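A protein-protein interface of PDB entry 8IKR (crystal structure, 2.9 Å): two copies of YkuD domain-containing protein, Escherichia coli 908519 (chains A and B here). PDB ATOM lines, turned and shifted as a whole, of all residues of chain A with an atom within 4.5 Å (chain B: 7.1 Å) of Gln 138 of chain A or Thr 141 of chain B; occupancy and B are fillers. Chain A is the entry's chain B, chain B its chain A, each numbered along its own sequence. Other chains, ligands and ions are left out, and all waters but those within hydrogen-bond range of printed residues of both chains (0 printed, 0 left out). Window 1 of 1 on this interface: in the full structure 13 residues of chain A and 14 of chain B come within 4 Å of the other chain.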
ATOM      1  N   MET A  22     -26.043 -11.300  13.972  1.00  0.00           N
ATOM      2  CA  MET A  22     -24.759 -11.601  13.377  1.00  0.00           C
ATOM      3  C   MET A  22     -23.663 -11.132  14.335  1.00  0.00           C
ATOM      4  O   MET A  22     -23.789 -10.065  14.926  1.00  0.00           O
ATOM      5  CB  MET A  22     -24.617 -10.874  12.038  1.00  0.00           C
ATOM      6  CG  MET A  22     -23.505 -11.417  11.199  1.00  0.00           C
ATOM      7  SD  MET A  22     -23.888 -11.610   9.436  1.00  0.00           S
ATOM      8  CE  MET A  22     -25.619 -12.095   9.406  1.00  0.00           C
ATOM      9  N   ASP A 134     -23.164 -20.936   3.348  1.00  0.00           N
ATOM     10  CA  ASP A 134     -23.163 -19.480   3.244  1.00  0.00           C
ATOM     11  C   ASP A 134     -23.590 -18.904   4.589  1.00  0.00           C
ATOM     12  O   ASP A 134     -22.885 -18.057   5.138  1.00  0.00           O
ATOM     13  CB  ASP A 134     -24.042 -18.959   2.095  1.00  0.00           C
ATOM     14  CG  ASP A 134     -23.529 -19.233   0.672  1.00  0.00           C
ATOM     15  OD1 ASP A 134     -22.304 -19.441   0.497  1.00  0.00           O
ATOM     16  OD2 ASP A 134     -24.344 -19.257  -0.294  1.00  0.00           O
ATOM     17  N   GLU A 135     -24.709 -19.428   5.117  1.00  0.00           N
ATOM     18  CA  GLU A 135     -25.360 -18.887   6.305  1.00  0.00           C
ATOM     19  C   GLU A 135     -24.439 -19.124   7.502  1.00  0.00           C
ATOM     20  O   GLU A 135     -24.190 -18.221   8.306  1.00  0.00           O
ATOM     21  CB  GLU A 135     -26.774 -19.465   6.494  1.00  0.00           C
ATOM     22  CG  GLU A 135     -27.825 -18.450   6.985  1.00  0.00           C
ATOM     23  CD  GLU A 135     -29.205 -18.984   7.415  1.00  0.00           C
ATOM     24  OE1 GLU A 135     -29.742 -18.572   8.512  1.00  0.00           O
ATOM     25  OE2 GLU A 135     -29.787 -19.815   6.649  1.00  0.00           O
ATOM     26  N   ILE A 136     -23.869 -20.330   7.557  1.00  0.00           N
ATOM     27  CA  ILE A 136     -23.034 -20.727   8.668  1.00  0.00           C
ATOM     28  C   ILE A 136     -21.774 -19.883   8.705  1.00  0.00           C
ATOM     29  O   ILE A 136     -21.479 -19.251   9.724  1.00  0.00           O
ATOM     30  CB  ILE A 136     -22.699 -22.224   8.580  1.00  0.00           C
ATOM     31  CG1 ILE A 136     -23.948 -23.074   8.862  1.00  0.00           C
ATOM     32  CG2 ILE A 136     -21.538 -22.525   9.527  1.00  0.00           C
ATOM     33  CD1 ILE A 136     -23.808 -24.545   8.575  1.00  0.00           C
ATOM     34  N   PHE A 137     -21.048 -19.904   7.585  1.00  0.00           N
ATOM     35  CA  PHE A 137     -19.721 -19.316   7.494  1.00  0.00           C
ATOM     36  C   PHE A 137     -19.781 -17.837   7.886  1.00  0.00           C
ATOM     37  O   PHE A 137     -18.863 -17.308   8.516  1.00  0.00           O
ATOM     38  CB  PHE A 137     -19.198 -19.563   6.077  1.00  0.00           C
ATOM     39  CG  PHE A 137     -17.736 -19.305   5.780  1.00  0.00           C
ATOM     40  CD1 PHE A 137     -17.200 -18.041   5.726  1.00  0.00           C
ATOM     41  CD2 PHE A 137     -16.900 -20.337   5.411  1.00  0.00           C
ATOM     42  CE1 PHE A 137     -15.866 -17.843   5.401  1.00  0.00           C
ATOM     43  CE2 PHE A 137     -15.571 -20.130   5.067  1.00  0.00           C
ATOM     44  CZ  PHE A 137     -15.052 -18.880   5.060  1.00  0.00           C
ATOM     45  N   GLN A 138     -20.871 -17.170   7.513  1.00  0.00           N
ATOM     46  CA  GLN A 138     -21.020 -15.741   7.774  1.00  0.00           C
ATOM     47  C   GLN A 138     -21.135 -15.482   9.281  1.00  0.00           C
ATOM     48  O   GLN A 138     -20.619 -14.480   9.778  1.00  0.00           O
ATOM     49  CB  GLN A 138     -22.223 -15.177   7.002  1.00  0.00           C
ATOM     50  CG  GLN A 138     -22.533 -13.734   7.330  1.00  0.00           C
ATOM     51  CD  GLN A 138     -21.548 -12.812   6.654  1.00  0.00           C
ATOM     52  OE1 GLN A 138     -21.686 -12.472   5.475  1.00  0.00           O
ATOM     53  NE2 GLN A 138     -20.562 -12.353   7.405  1.00  0.00           N
ATOM     54  N   PHE A 139     -21.824 -16.387   9.987  1.00  0.00           N
ATOM     55  CA  PHE A 139     -22.139 -16.175  11.392  1.00  0.00           C
ATOM     56  C   PHE A 139     -20.933 -16.453  12.267  1.00  0.00           C
ATOM     57  O   PHE A 139     -20.755 -15.806  13.303  1.00  0.00           O
ATOM     58  CB  PHE A 139     -23.270 -17.092  11.817  1.00  0.00           C
ATOM     59  CG  PHE A 139     -24.569 -16.369  11.880  1.00  0.00           C
ATOM     60  CD1 PHE A 139     -24.867 -15.602  12.984  1.00  0.00           C
ATOM     61  CD2 PHE A 139     -25.441 -16.403  10.810  1.00  0.00           C
ATOM     62  CE1 PHE A 139     -26.064 -14.902  13.028  1.00  0.00           C
ATOM     63  CE2 PHE A 139     -26.629 -15.699  10.844  1.00  0.00           C
ATOM     64  CZ  PHE A 139     -26.934 -14.942  11.950  1.00  0.00           C
ATOM     65  N   VAL A 140     -20.164 -17.444  11.809  1.00  0.00           N
ATOM     66  CA  VAL A 140     -18.911 -17.787  12.435  1.00  0.00           C
ATOM     67  C   VAL A 140     -17.986 -16.587  12.291  1.00  0.00           C
ATOM     68  O   VAL A 140     -17.581 -16.005  13.293  1.00  0.00           O
ATOM     69  CB  VAL A 140     -18.292 -19.055  11.834  1.00  0.00           C
ATOM     70  CG1 VAL A 140     -16.969 -19.367  12.485  1.00  0.00           C
ATOM     71  CG2 VAL A 140     -19.219 -20.232  11.969  1.00  0.00           C
ATOM     72  N   THR A 141     -17.661 -16.208  11.042  1.00  0.00           N
ATOM     73  CA  THR A 141     -16.722 -15.112  10.828  1.00  0.00           C
ATOM     74  C   THR A 141     -17.232 -13.893  11.579  1.00  0.00           C
ATOM     75  O   THR A 141     -16.456 -13.124  12.147  1.00  0.00           O
ATOM     76  CB  THR A 141     -16.504 -14.781   9.357  1.00  0.00           C
ATOM     77  OG1 THR A 141     -17.809 -14.617   8.837  1.00  0.00           O
ATOM     78  CG2 THR A 141     -15.838 -15.855   8.550  1.00  0.00           C
ATOM     79  N   GLY A 142     -18.551 -13.747  11.614  1.00  0.00           N
ATOM     80  CA  GLY A 142     -19.167 -12.703  12.409  1.00  0.00           C
ATOM     81  C   GLY A 142     -18.683 -12.743  13.841  1.00  0.00           C
ATOM     82  O   GLY A 142     -18.081 -11.789  14.308  1.00  0.00           O
ATOM     83  N   VAL A 145     -14.951 -12.032  14.178  1.00  0.00           N
ATOM     84  CA  VAL A 145     -14.644 -10.620  14.076  1.00  0.00           C
ATOM     85  C   VAL A 145     -14.840  -9.953  15.439  1.00  0.00           C
ATOM     86  O   VAL A 145     -13.965  -9.214  15.858  1.00  0.00           O
ATOM     87  CB  VAL A 145     -15.455  -9.922  12.964  1.00  0.00           C
ATOM     88  CG1 VAL A 145     -15.746  -8.484  13.260  1.00  0.00           C
ATOM     89  CG2 VAL A 145     -14.748  -9.960  11.640  1.00  0.00           C
ATOM     90  N   MET B  22     -11.853 -15.062  -0.541  1.00  0.00           N
ATOM     91  CA  MET B  22     -12.388 -14.510   0.683  1.00  0.00           C
ATOM     92  C   MET B  22     -11.236 -14.210   1.624  1.00  0.00           C
ATOM     93  O   MET B  22     -10.301 -14.983   1.689  1.00  0.00           O
ATOM     94  CB  MET B  22     -13.327 -15.529   1.299  1.00  0.00           C
ATOM     95  CG  MET B  22     -14.139 -15.036   2.456  1.00  0.00           C
ATOM     96  SD  MET B  22     -15.788 -14.629   1.941  1.00  0.00           S
ATOM     97  CE  MET B  22     -16.172 -16.010   0.852  1.00  0.00           C
ATOM     98  N   GLY B  23     -11.277 -13.047   2.290  1.00  0.00           N
ATOM     99  CA  GLY B  23     -10.349 -12.765   3.382  1.00  0.00           C
ATOM    100  C   GLY B  23      -9.084 -12.068   2.891  1.00  0.00           C
ATOM    101  O   GLY B  23      -8.290 -11.556   3.699  1.00  0.00           O
ATOM    102  N   GLN B  81     -14.127  -0.565   9.703  1.00  0.00           N
ATOM    103  CA  GLN B  81     -13.497  -1.519  10.627  1.00  0.00           C
ATOM    104  C   GLN B  81     -14.497  -2.495  11.277  1.00  0.00           C
ATOM    105  O   GLN B  81     -14.842  -3.483  10.645  1.00  0.00           O
ATOM    106  CB  GLN B  81     -12.682  -0.767  11.654  1.00  0.00           C
ATOM    107  CG  GLN B  81     -11.656   0.160  11.037  1.00  0.00           C
ATOM    108  CD  GLN B  81     -10.869   0.794  12.154  1.00  0.00           C
ATOM    109  OE1 GLN B  81     -11.374   0.966  13.262  1.00  0.00           O
ATOM    110  NE2 GLN B  81      -9.624   1.141  11.892  1.00  0.00           N
ATOM    111  N   GLN B  84     -19.600  -2.886  11.476  1.00  0.00           N
ATOM    112  CA  GLN B  84     -20.670  -3.795  11.031  1.00  0.00           C
ATOM    113  C   GLN B  84     -21.524  -4.210  12.212  1.00  0.00           C
ATOM    114  O   GLN B  84     -22.419  -5.031  12.072  1.00  0.00           O
ATOM    115  CB  GLN B  84     -20.322  -5.148  10.395  1.00  0.00           C
ATOM    116  CG  GLN B  84     -18.876  -5.558  10.524  1.00  0.00           C
ATOM    117  CD  GLN B  84     -18.128  -5.015   9.339  1.00  0.00           C
ATOM    118  OE1 GLN B  84     -16.931  -4.762   9.383  1.00  0.00           O
ATOM    119  NE2 GLN B  84     -18.849  -4.825   8.251  1.00  0.00           N
ATOM    120  N   LYS B  86     -24.538  -4.550  14.224  1.00  0.00           N
ATOM    121  CA  LYS B  86     -25.856  -4.478  13.626  1.00  0.00           C
ATOM    122  C   LYS B  86     -26.698  -3.334  14.225  1.00  0.00           C
ATOM    123  O   LYS B  86     -26.952  -3.317  15.423  1.00  0.00           O
ATOM    124  CB  LYS B  86     -26.435  -5.874  13.823  1.00  0.00           C
ATOM    125  CG  LYS B  86     -25.651  -6.946  13.081  1.00  0.00           C
ATOM    126  CD  LYS B  86     -25.671  -6.821  11.503  1.00  0.00           C
ATOM    127  CE  LYS B  86     -25.698  -8.162  10.764  1.00  0.00           C
ATOM    128  NZ  LYS B  86     -26.275  -8.145   9.410  1.00  0.00           N
ATOM    129  N   LYS B  93     -27.790  -5.774   7.066  1.00  0.00           N
ATOM    130  CA  LYS B  93     -26.371  -5.915   6.809  1.00  0.00           C
ATOM    131  C   LYS B  93     -25.752  -4.540   6.618  1.00  0.00           C
ATOM    132  O   LYS B  93     -25.070  -4.305   5.652  1.00  0.00           O
ATOM    133  CB  LYS B  93     -26.103  -6.887   5.659  1.00  0.00           C
ATOM    134  CG  LYS B  93     -26.366  -8.354   5.956  1.00  0.00           C
ATOM    135  CD  LYS B  93     -25.443  -9.272   5.178  1.00  0.00           C
ATOM    136  CE  LYS B  93     -25.518 -10.753   5.500  1.00  0.00           C
ATOM    137  NZ  LYS B  93     -26.660 -11.386   4.831  1.00  0.00           N
ATOM    138  N   ILE B 133     -25.676  -7.188  -0.991  1.00  0.00           N
ATOM    139  CA  ILE B 133     -25.061  -6.866   0.269  1.00  0.00           C
ATOM    140  C   ILE B 133     -24.465  -8.161   0.845  1.00  0.00           C
ATOM    141  O   ILE B 133     -23.369  -8.139   1.422  1.00  0.00           O
ATOM    142  CB  ILE B 133     -26.094  -6.177   1.171  1.00  0.00           C
ATOM    143  CG1 ILE B 133     -25.444  -5.619   2.429  1.00  0.00           C
ATOM    144  CG2 ILE B 133     -27.221  -7.120   1.516  1.00  0.00           C
ATOM    145  CD1 ILE B 133     -24.555  -4.432   2.157  1.00  0.00           C
ATOM    146  N   ASP B 134     -25.154  -9.298   0.654  1.00  0.00           N
ATOM    147  CA  ASP B 134     -24.664 -10.568   1.184  1.00  0.00           C
ATOM    148  C   ASP B 134     -23.220 -10.734   0.734  1.00  0.00           C
ATOM    149  O   ASP B 134     -22.321 -10.974   1.541  1.00  0.00           O
ATOM    150  CB  ASP B 134     -25.547 -11.773   0.802  1.00  0.00           C
ATOM    151  CG  ASP B 134     -26.953 -11.810   1.428  1.00  0.00           C
ATOM    152  OD1 ASP B 134     -27.105 -11.357   2.570  1.00  0.00           O
ATOM    153  OD2 ASP B 134     -27.920 -12.303   0.777  1.00  0.00           O
ATOM    154  N   GLU B 135     -23.014 -10.545  -0.570  1.00  0.00           N
ATOM    155  CA  GLU B 135     -21.738 -10.860  -1.192  1.00  0.00           C
ATOM    156  C   GLU B 135     -20.685  -9.891  -0.648  1.00  0.00           C
ATOM    157  O   GLU B 135     -19.587 -10.324  -0.267  1.00  0.00           O
ATOM    158  CB  GLU B 135     -21.905 -10.860  -2.716  1.00  0.00           C
ATOM    159  CG  GLU B 135     -21.134 -11.973  -3.423  1.00  0.00           C
ATOM    160  CD  GLU B 135     -21.038 -11.750  -4.931  1.00  0.00           C
ATOM    161  OE1 GLU B 135     -22.107 -11.653  -5.593  1.00  0.00           O
ATOM    162  OE2 GLU B 135     -19.892 -11.645  -5.457  1.00  0.00           O
ATOM    163  N   ILE B 136     -21.056  -8.595  -0.575  1.00  0.00           N
ATOM    164  CA  ILE B 136     -20.163  -7.532  -0.126  1.00  0.00           C
ATOM    165  C   ILE B 136     -19.712  -7.781   1.306  1.00  0.00           C
ATOM    166  O   ILE B 136     -18.526  -7.863   1.581  1.00  0.00           O
ATOM    167  CB  ILE B 136     -20.867  -6.160  -0.192  1.00  0.00           C
ATOM    168  CG1 ILE B 136     -21.139  -5.745  -1.639  1.00  0.00           C
ATOM    169  CG2 ILE B 136     -20.046  -5.120   0.558  1.00  0.00           C
ATOM    170  CD1 ILE B 136     -22.039  -4.574  -1.744  1.00  0.00           C
ATOM    171  N   PHE B 137     -20.694  -7.900   2.194  1.00  0.00           N
ATOM    172  CA  PHE B 137     -20.485  -7.911   3.633  1.00  0.00           C
ATOM    173  C   PHE B 137     -19.577  -9.078   4.035  1.00  0.00           C
ATOM    174  O   PHE B 137     -18.757  -8.964   4.942  1.00  0.00           O
ATOM    175  CB  PHE B 137     -21.855  -8.055   4.297  1.00  0.00           C
ATOM    176  CG  PHE B 137     -21.969  -7.723   5.762  1.00  0.00           C
ATOM    177  CD1 PHE B 137     -22.214  -6.435   6.158  1.00  0.00           C
ATOM    178  CD2 PHE B 137     -21.901  -8.689   6.739  1.00  0.00           C
ATOM    179  CE1 PHE B 137     -22.381  -6.124   7.497  1.00  0.00           C
ATOM    180  CE2 PHE B 137     -22.068  -8.370   8.071  1.00  0.00           C
ATOM    181  CZ  PHE B 137     -22.331  -7.095   8.461  1.00  0.00           C
ATOM    182  N   GLN B 138     -19.713 -10.209   3.336  1.00  0.00           N
ATOM    183  CA  GLN B 138     -18.916 -11.369   3.667  1.00  0.00           C
ATOM    184  C   GLN B 138     -17.457 -11.127   3.322  1.00  0.00           C
ATOM    185  O   GLN B 138     -16.576 -11.625   4.021  1.00  0.00           O
ATOM    186  CB  GLN B 138     -19.402 -12.596   2.902  1.00  0.00           C
ATOM    187  CG  GLN B 138     -18.645 -13.873   3.239  1.00  0.00           C
ATOM    188  CD  GLN B 138     -18.961 -14.354   4.634  1.00  0.00           C
ATOM    189  OE1 GLN B 138     -18.458 -13.813   5.611  1.00  0.00           O
ATOM    190  NE2 GLN B 138     -19.768 -15.393   4.744  1.00  0.00           N
ATOM    191  N   PHE B 139     -17.220 -10.384   2.233  1.00  0.00           N
ATOM    192  CA  PHE B 139     -15.880 -10.197   1.703  1.00  0.00           C
ATOM    193  C   PHE B 139     -15.131  -9.202   2.560  1.00  0.00           C
ATOM    194  O   PHE B 139     -13.898  -9.319   2.711  1.00  0.00           O
ATOM    195  CB  PHE B 139     -15.929  -9.748   0.249  1.00  0.00           C
ATOM    196  CG  PHE B 139     -15.660 -10.882  -0.696  1.00  0.00           C
ATOM    197  CD1 PHE B 139     -14.371 -11.347  -0.882  1.00  0.00           C
ATOM    198  CD2 PHE B 139     -16.702 -11.551  -1.313  1.00  0.00           C
ATOM    199  CE1 PHE B 139     -14.126 -12.373  -1.791  1.00  0.00           C
ATOM    200  CE2 PHE B 139     -16.459 -12.586  -2.211  1.00  0.00           C
ATOM    201  CZ  PHE B 139     -15.171 -12.992  -2.445  1.00  0.00           C
ATOM    202  N   VAL B 140     -15.920  -8.252   3.064  1.00  0.00           N
ATOM    203  CA  VAL B 140     -15.427  -7.253   3.987  1.00  0.00           C
ATOM    204  C   VAL B 140     -15.010  -7.956   5.278  1.00  0.00           C
ATOM    205  O   VAL B 140     -13.838  -7.936   5.656  1.00  0.00           O
ATOM    206  CB  VAL B 140     -16.458  -6.131   4.226  1.00  0.00           C
ATOM    207  CG1 VAL B 140     -16.036  -5.183   5.350  1.00  0.00           C
ATOM    208  CG2 VAL B 140     -16.723  -5.362   2.948  1.00  0.00           C
ATOM    209  N   THR B 141     -15.972  -8.582   5.963  1.00  0.00           N
ATOM    210  CA  THR B 141     -15.681  -9.223   7.236  1.00  0.00           C
ATOM    211  C   THR B 141     -14.506 -10.178   7.040  1.00  0.00           C
ATOM    212  O   THR B 141     -13.592 -10.203   7.869  1.00  0.00           O
ATOM    213  CB  THR B 141     -16.927  -9.921   7.795  1.00  0.00           C
ATOM    214  OG1 THR B 141     -17.330 -10.863   6.797  1.00  0.00           O
ATOM    215  CG2 THR B 141     -18.061  -8.963   8.140  1.00  0.00           C
ATOM    216  N   GLY B 142     -14.523 -10.906   5.904  1.00  0.00           N
ATOM    217  CA  GLY B 142     -13.402 -11.717   5.451  1.00  0.00           C
ATOM    218  C   GLY B 142     -12.076 -10.984   5.623  1.00  0.00           C
ATOM    219  O   GLY B 142     -11.226 -11.372   6.412  1.00  0.00           O
ATOM    220  N   ALA B 143     -11.934  -9.893   4.877  1.00  0.00           N
ATOM    221  CA  ALA B 143     -10.717  -9.091   4.855  1.00  0.00           C
ATOM    222  C   ALA B 143     -10.254  -8.702   6.268  1.00  0.00           C
ATOM    223  O   ALA B 143      -9.065  -8.823   6.579  1.00  0.00           O
ATOM    224  CB  ALA B 143     -10.942  -7.866   3.978  1.00  0.00           C
ATOM    225  N   LEU B 144     -11.194  -8.234   7.109  1.00  0.00           N
ATOM    226  CA  LEU B 144     -10.874  -7.728   8.439  1.00  0.00           C
ATOM    227  C   LEU B 144     -10.443  -8.876   9.333  1.00  0.00           C
ATOM    228  O   LEU B 144      -9.479  -8.740  10.087  1.00  0.00           O
ATOM    229  CB  LEU B 144     -12.081  -7.004   9.048  1.00  0.00           C
ATOM    230  CG  LEU B 144     -12.463  -5.664   8.392  1.00  0.00           C
ATOM    231  CD1 LEU B 144     -13.898  -5.381   8.571  1.00  0.00           C
ATOM    232  CD2 LEU B 144     -11.732  -4.472   8.947  1.00  0.00           C
ATOM    233  N   VAL B 145     -11.131 -10.016   9.209  1.00  0.00           N
ATOM    234  CA  VAL B 145     -10.697 -11.193   9.946  1.00  0.00           C
ATOM    235  C   VAL B 145      -9.194 -11.376   9.732  1.00  0.00           C
ATOM    236  O   VAL B 145      -8.468 -11.575  10.708  1.00  0.00           O
ATOM    237  CB  VAL B 145     -11.477 -12.461   9.567  1.00  0.00           C
ATOM    238  CG1 VAL B 145     -10.641 -13.699   9.855  1.00  0.00           C
ATOM    239  CG2 VAL B 145     -12.822 -12.540  10.282  1.00  0.00           C
ATOM    240  N   PHE B 146      -8.731 -11.337   8.472  1.00  0.00           N
ATOM    241  CA  PHE B 146      -7.331 -11.563   8.145  1.00  0.00           C
ATOM    242  C   PHE B 146      -6.624 -10.234   7.969  1.00  0.00           C
ATOM    243  O   PHE B 146      -6.526  -9.734   6.850  1.00  0.00           O
ATOM    244  CB  PHE B 146      -7.209 -12.417   6.880  1.00  0.00           C
ATOM    245  CG  PHE B 146      -7.779 -13.803   7.039  1.00  0.00           C
ATOM    246  CD1 PHE B 146      -7.028 -14.819   7.649  1.00  0.00           C
ATOM    247  CD2 PHE B 146      -9.086 -14.084   6.636  1.00  0.00           C
ATOM    248  CE1 PHE B 146      -7.554 -16.092   7.827  1.00  0.00           C
ATOM    249  CE2 PHE B 146      -9.612 -15.361   6.831  1.00  0.00           C
ATOM    250  CZ  PHE B 146      -8.854 -16.355   7.431  1.00  0.00           C
ATOM    251  N   VAL B 151     -10.996  -1.266   5.538  1.00  0.00           N
ATOM    252  CA  VAL B 151     -11.388  -1.227   4.141  1.00  0.00           C
ATOM    253  C   VAL B 151     -11.638   0.225   3.768  1.00  0.00           C
ATOM    254  O   VAL B 151     -12.460   0.888   4.396  1.00  0.00           O
ATOM    255  CB  VAL B 151     -12.662  -2.042   3.895  1.00  0.00           C
ATOM    256  CG1 VAL B 151     -13.085  -2.028   2.437  1.00  0.00           C
ATOM    257  CG2 VAL B 151     -12.480  -3.462   4.369  1.00  0.00           C
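Of chain B, only Phe 137 (3.96 Å), Gln 138 (3.1 Å) and Thr 141 (3.6 Å) come within 4 Å of Gln 138 of chain A. Of chain A, only Gln 138 (3.6 Å) and Val 145 (3.95 Å) come within 4 Å of Thr 141 of chain B. Of the printed residues of chain A, Lys 86 of chain B touches Met 22. Of the printed residues of chain B, Phe 137 of chain A touches Gln 138 (3.8 Å). Of the printed residues of chain B, Thr 141 of chain A touches Gln 138 (3.4 Å). Phe 146 of chain B touches none of the printed residues of chain A. Phe 139 of chain A touches none of the printed residues of chain B. The nearest residue of chain A that does not touch Thr 141 of chain B is Thr 141 of chain A (4.3 Å). The nearest printed residue of chain A that does not touch Phe 137 of chain B is Gly 142 of chain A (6.8 Å).
Hydrophobic or aromatic side chains of chain B that line the printed part of chain A: Phe 137 and Val 145. Among the printed residues, 9 pairs touch across the chains.
The side-chain hydroxyl (OG1) of Thr 141 of chain B sits at hydrogen-bond distance from the backbone carbonyl oxygen (O) of Phe 137 of chain B (3.0 Å). The backbone carbonyl oxygen of Gln 138 of chain B is in hydrogen-bond range of the side-chain hydroxyl of Thr 141 of chain B, at 3.0 Å. The backbone carbonyl oxygen of Phe 137 of chain A is in hydrogen-bond range of the side-chain hydroxyl of Thr 141 of chain A (2.9 Å). The backbone carbonyl oxygen (O) of Gln 138 of chain A sits at hydrogen-bond distance from the side-chain hydroxyl (OG1) of Thr 141 of chain A (3.0 Å).
Met 22 of chain A touches Phe 137 of chain B, but with the chains exchanged Phe 137 of chain A does not touch Met 22 of chain B (4.4 Å). Phe 137 of chain A touches Gln 138 of chain B, and with the chains exchanged Gln 138 of chain A touches Phe 137 of chain B. Val 145 of chain A touches Thr 141 of chain B, but with the chains exchanged Thr 141 of chain A does not touch Val 145 of chain B (4.1 Å). Val 145 of chain A touches its own counterpart, Val 145 of chain B. Positions printed for both chains: 22, 134, 135, 136, 137, 138, 139, 140, 141, 142 and 145.
Among the printed residues, pairs that only touch across the chains: Met 22 of chain A with Lys 86 of chain B, Val 145 of chain A with Val 145 of chain B, Gln 138 of chain A with Thr 141 of chain B, Phe 137 of chain A with Gln 138 of chain B, Val 145 of chain A with Thr 141 of chain B, Gln 138 of chain A with Phe 137 of chain B and Met 22 of chain A with Phe 137 of chain B.
OE1 of Gln 138 of chain B sits at hydrogen-bond distance from NE2 of Gln 138 of chain A (3.1 Å). The side-chain amide oxygen (OE1) of Gln 138 of chain B sits at hydrogen-bond distance from the side-chain hydroxyl (OG1) of Thr 141 of chain A, 3.4 Å away.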
